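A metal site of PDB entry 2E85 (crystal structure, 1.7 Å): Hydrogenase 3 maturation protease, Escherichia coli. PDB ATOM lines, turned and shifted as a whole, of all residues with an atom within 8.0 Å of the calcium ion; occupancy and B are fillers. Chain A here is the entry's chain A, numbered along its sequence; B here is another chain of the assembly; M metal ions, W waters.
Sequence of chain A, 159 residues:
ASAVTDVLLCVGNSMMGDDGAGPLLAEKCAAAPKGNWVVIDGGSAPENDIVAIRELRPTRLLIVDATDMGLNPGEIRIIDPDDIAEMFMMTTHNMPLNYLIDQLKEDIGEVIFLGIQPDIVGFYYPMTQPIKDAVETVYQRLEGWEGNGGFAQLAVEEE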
ATOM      1  N   LEU A   9     -25.753  24.599   5.484  1.00  0.00           N
ATOM      2  CA  LEU A   9     -25.343  23.898   6.709  1.00  0.00           C
ATOM      3  C   LEU A   9     -24.983  22.467   6.355  1.00  0.00           C
ATOM      4  O   LEU A   9     -25.838  21.718   5.835  1.00  0.00           O
ATOM      5  CB  LEU A   9     -26.460  23.933   7.729  1.00  0.00           C
ATOM      6  CG  LEU A   9     -26.192  23.107   8.990  1.00  0.00           C
ATOM      7  CD1 LEU A   9     -25.007  23.629   9.816  1.00  0.00           C
ATOM      8  CD2 LEU A   9     -27.450  23.010   9.837  1.00  0.00           C
ATOM      9  N   CYS A  10     -23.719  22.094   6.572  1.00  0.00           N
ATOM     10  CA  CYS A  10     -23.281  20.723   6.272  1.00  0.00           C
ATOM     11  C   CYS A  10     -23.293  19.905   7.554  1.00  0.00           C
ATOM     12  O   CYS A  10     -22.645  20.288   8.552  1.00  0.00           O
ATOM     13  CB  CYS A  10     -21.869  20.694   5.671  1.00  0.00           C
ATOM     14  SG  CYS A  10     -21.810  21.404   4.017  1.00  0.00           S
ATOM     15  N   VAL A  11     -24.051  18.804   7.549  1.00  0.00           N
ATOM     16  CA  VAL A  11     -24.204  18.010   8.778  1.00  0.00           C
ATOM     17  C   VAL A  11     -23.539  16.626   8.604  1.00  0.00           C
ATOM     18  O   VAL A  11     -23.693  15.975   7.573  1.00  0.00           O
ATOM     19  CB  VAL A  11     -25.697  17.852   9.222  1.00  0.00           C
ATOM     20  CG1 VAL A  11     -25.844  16.942  10.466  1.00  0.00           C
ATOM     21  CG2 VAL A  11     -26.319  19.211   9.531  1.00  0.00           C
ATOM     22  N   GLY A  12     -22.801  16.178   9.626  1.00  0.00           N
ATOM     23  CA  GLY A  12     -22.190  14.851   9.525  1.00  0.00           C
ATOM     24  C   GLY A  12     -20.965  14.682  10.398  1.00  0.00           C
ATOM     25  O   GLY A  12     -20.517  15.613  11.076  1.00  0.00           O
ATOM     26  N   ILE A  40     -21.454  26.425   6.634  1.00  0.00           N
ATOM     27  CA  ILE A  40     -21.199  26.067   8.038  1.00  0.00           C
ATOM     28  C   ILE A  40     -20.889  24.563   8.088  1.00  0.00           C
ATOM     29  O   ILE A  40     -21.705  23.707   7.681  1.00  0.00           O
ATOM     30  CB  ILE A  40     -22.400  26.410   8.935  1.00  0.00           C
ATOM     31  CG1 ILE A  40     -22.553  27.954   8.963  1.00  0.00           C
ATOM     32  CG2 ILE A  40     -22.272  25.879  10.313  1.00  0.00           C
ATOM     33  CD1 ILE A  40     -21.377  28.779   9.568  1.00  0.00           C
ATOM     34  N   ASP A  41     -19.695  24.262   8.604  1.00  0.00           N
ATOM     35  CA  ASP A  41     -19.204  22.931   8.851  1.00  0.00           C
ATOM     36  C   ASP A  41     -19.800  22.457  10.183  1.00  0.00           C
ATOM     37  O   ASP A  41     -19.132  22.484  11.214  1.00  0.00           O
ATOM     38  CB  ASP A  41     -17.679  23.004   8.888  1.00  0.00           C
ATOM     39  CG  ASP A  41     -16.968  21.650   8.738  1.00  0.00           C
ATOM     40  OD1 ASP A  41     -17.641  20.605   8.619  1.00  0.00           O
ATOM     41  OD2 ASP A  41     -15.705  21.671   8.759  1.00  0.00           O
ATOM     42  N   GLY A  42     -21.065  22.050  10.149  1.00  0.00           N
ATOM     43  CA  GLY A  42     -21.852  21.859  11.354  1.00  0.00           C
ATOM     44  C   GLY A  42     -21.578  20.625  12.210  1.00  0.00           C
ATOM     45  O   GLY A  42     -22.130  20.493  13.317  1.00  0.00           O
ATOM     46  N   GLY A  43     -20.784  19.685  11.705  1.00  0.00           N
ATOM     47  CA  GLY A  43     -20.518  18.515  12.509  1.00  0.00           C
ATOM     48  C   GLY A  43     -21.740  17.643  12.806  1.00  0.00           C
ATOM     49  O   GLY A  43     -22.717  17.615  12.057  1.00  0.00           O
ATOM     50  N   SER A  44     -21.663  16.966  13.946  1.00  0.00           N
ATOM     51  CA  SER A  44     -22.584  15.921  14.322  1.00  0.00           C
ATOM     52  C   SER A  44     -24.003  16.380  14.608  1.00  0.00           C
ATOM     53  O   SER A  44     -24.955  15.651  14.346  1.00  0.00           O
ATOM     54  CB  SER A  44     -22.016  15.180  15.546  1.00  0.00           C
ATOM     55  OG  SER A  44     -20.826  14.502  15.193  1.00  0.00           O
ATOM     56  N   ALA A  45     -24.139  17.598  15.139  1.00  0.00           N
ATOM     57  CA  ALA A  45     -25.437  18.079  15.621  1.00  0.00           C
ATOM     58  C   ALA A  45     -25.716  19.464  15.088  1.00  0.00           C
ATOM     59  O   ALA A  45     -24.869  20.355  15.205  1.00  0.00           O
ATOM     60  CB  ALA A  45     -25.475  18.080  17.140  1.00  0.00           C
ATOM     61  N   PRO A  46     -26.910  19.670  14.502  1.00  0.00           N
ATOM     62  CA  PRO A  46     -27.268  21.015  14.042  1.00  0.00           C
ATOM     63  C   PRO A  46     -27.706  21.977  15.172  1.00  0.00           C
ATOM     64  O   PRO A  46     -27.716  23.198  14.968  1.00  0.00           O
ATOM     65  CB  PRO A  46     -28.449  20.732  13.087  1.00  0.00           C
ATOM     66  CG  PRO A  46     -29.099  19.516  13.730  1.00  0.00           C
ATOM     67  CD  PRO A  46     -27.969  18.678  14.209  1.00  0.00           C
ATOM     68  N   GLU A  47     -28.037  21.447  16.351  1.00  0.00           N
ATOM     69  CA  GLU A  47     -28.559  22.287  17.460  1.00  0.00           C
ATOM     70  C   GLU A  47     -27.690  23.480  17.767  1.00  0.00           C
ATOM     71  O   GLU A  47     -28.182  24.598  17.951  1.00  0.00           O
ATOM     72  CB  GLU A  47     -28.750  21.481  18.746  1.00  0.00           C
ATOM     73  CG  GLU A  47     -29.992  20.651  18.782  1.00  0.00           C
ATOM     74  CD  GLU A  47     -29.757  19.234  18.261  1.00  0.00           C
ATOM     75  OE1 GLU A  47     -28.912  19.025  17.338  1.00  0.00           O
ATOM     76  OE2 GLU A  47     -30.443  18.327  18.764  1.00  0.00           O
ATOM     77  N   ASN A  48     -26.392  23.253  17.806  1.00  0.00           N
ATOM     78  CA  ASN A  48     -25.507  24.315  18.243  1.00  0.00           C
ATOM     79  C   ASN A  48     -25.060  25.214  17.087  1.00  0.00           C
ATOM     80  O   ASN A  48     -24.216  26.096  17.273  1.00  0.00           O
ATOM     81  CB  ASN A  48     -24.317  23.751  19.030  1.00  0.00           C
ATOM     82  CG  ASN A  48     -23.328  23.023  18.175  1.00  0.00           C
ATOM     83  OD1 ASN A  48     -23.690  22.455  17.146  1.00  0.00           O
ATOM     84  ND2 ASN A  48     -22.028  23.060  18.568  1.00  0.00           N
ATOM     85  N   ASP A  49     -25.668  25.031  15.915  1.00  0.00           N
ATOM     86  CA  ASP A  49     -25.349  25.854  14.731  1.00  0.00           C
ATOM     87  C   ASP A  49     -26.441  26.880  14.466  1.00  0.00           C
ATOM     88  O   ASP A  49     -26.302  27.776  13.617  1.00  0.00           O
ATOM     89  CB  ASP A  49     -25.173  24.959  13.488  1.00  0.00           C
ATOM     90  CG  ASP A  49     -24.196  23.816  13.723  1.00  0.00           C
ATOM     91  OD1 ASP A  49     -23.121  24.054  14.327  1.00  0.00           O
ATOM     92  OD2 ASP A  49     -24.507  22.658  13.321  1.00  0.00           O
ATOM     93  N   ILE A  50     -27.550  26.713  15.166  1.00  0.00           N
ATOM     94  CA  ILE A  50     -28.752  27.527  14.940  1.00  0.00           C
ATOM     95  C   ILE A  50     -28.522  29.024  15.203  1.00  0.00           C
ATOM     96  O   ILE A  50     -28.907  29.876  14.372  1.00  0.00           O
ATOM     97  CB  ILE A  50     -29.926  26.983  15.783  1.00  0.00           C
ATOM     98  CG1 ILE A  50     -30.394  25.629  15.256  1.00  0.00           C
ATOM     99  CG2 ILE A  50     -31.123  27.937  15.702  1.00  0.00           C
ATOM    100  CD1 ILE A  50     -31.342  24.866  16.141  1.00  0.00           C
ATOM    101  N   HIS A  93     -29.164  14.171  19.348  1.00  0.00           N
ATOM    102  CA  HIS A  93     -29.592  14.438  20.724  1.00  0.00           C
ATOM    103  C   HIS A  93     -31.055  14.085  20.937  1.00  0.00           C
ATOM    104  O   HIS A  93     -31.653  14.414  21.966  1.00  0.00           O
ATOM    105  CB  HIS A  93     -29.330  15.907  21.089  1.00  0.00           C
ATOM    106  CG  HIS A  93     -27.880  16.262  21.052  1.00  0.00           C
ATOM    107  ND1 HIS A  93     -26.922  15.552  21.748  1.00  0.00           N
ATOM    108  CD2 HIS A  93     -27.216  17.238  20.378  1.00  0.00           C
ATOM    109  CE1 HIS A  93     -25.732  16.080  21.501  1.00  0.00           C
ATOM    110  NE2 HIS A  93     -25.880  17.102  20.683  1.00  0.00           N
ATOM    111  N   HIS B  93     -27.289  21.458  25.164  1.00  0.00           N
ATOM    112  CA  HIS B  93     -26.703  21.092  23.861  1.00  0.00           C
ATOM    113  C   HIS B  93     -26.479  22.318  22.994  1.00  0.00           C
ATOM    114  O   HIS B  93     -26.210  22.215  21.780  1.00  0.00           O
ATOM    115  CB  HIS B  93     -27.594  20.068  23.134  1.00  0.00           C
ATOM    116  CG  HIS B  93     -27.760  18.793  23.906  1.00  0.00           C
ATOM    117  ND1 HIS B  93     -26.697  18.016  24.291  1.00  0.00           N
ATOM    118  CD2 HIS B  93     -28.881  18.159  24.360  1.00  0.00           C
ATOM    119  CE1 HIS B  93     -27.134  16.970  24.968  1.00  0.00           C
ATOM    120  NE2 HIS B  93     -28.446  17.028  25.017  1.00  0.00           N
HETATM  121 CA    CA M   1     -22.968  21.613  15.131  1.00  0.00          CA
HETATM  122  O   HOH W   1     -20.660  22.219  15.776  1.00  0.00           O
HETATM  123  O   HOH W   2     -22.140  19.606  16.374  1.00  0.00           O
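The calcium ion is bound by the backbone carbonyl oxygen (O) of Ala 45, the backbone carbonyl oxygen (O) of Gly 42, the side-chain amide oxygen (OD1) of Asn 48, water W1, water W2, the side-chain carboxylate (OD1) of Asp 49 and the side-chain carboxylate (OD2) of Asp 49.
The backbone carbonyl oxygen (O) of Cys 10 sits at hydrogen-bond distance from the backbone NH (N) of Gly 42 (2.9 Å).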
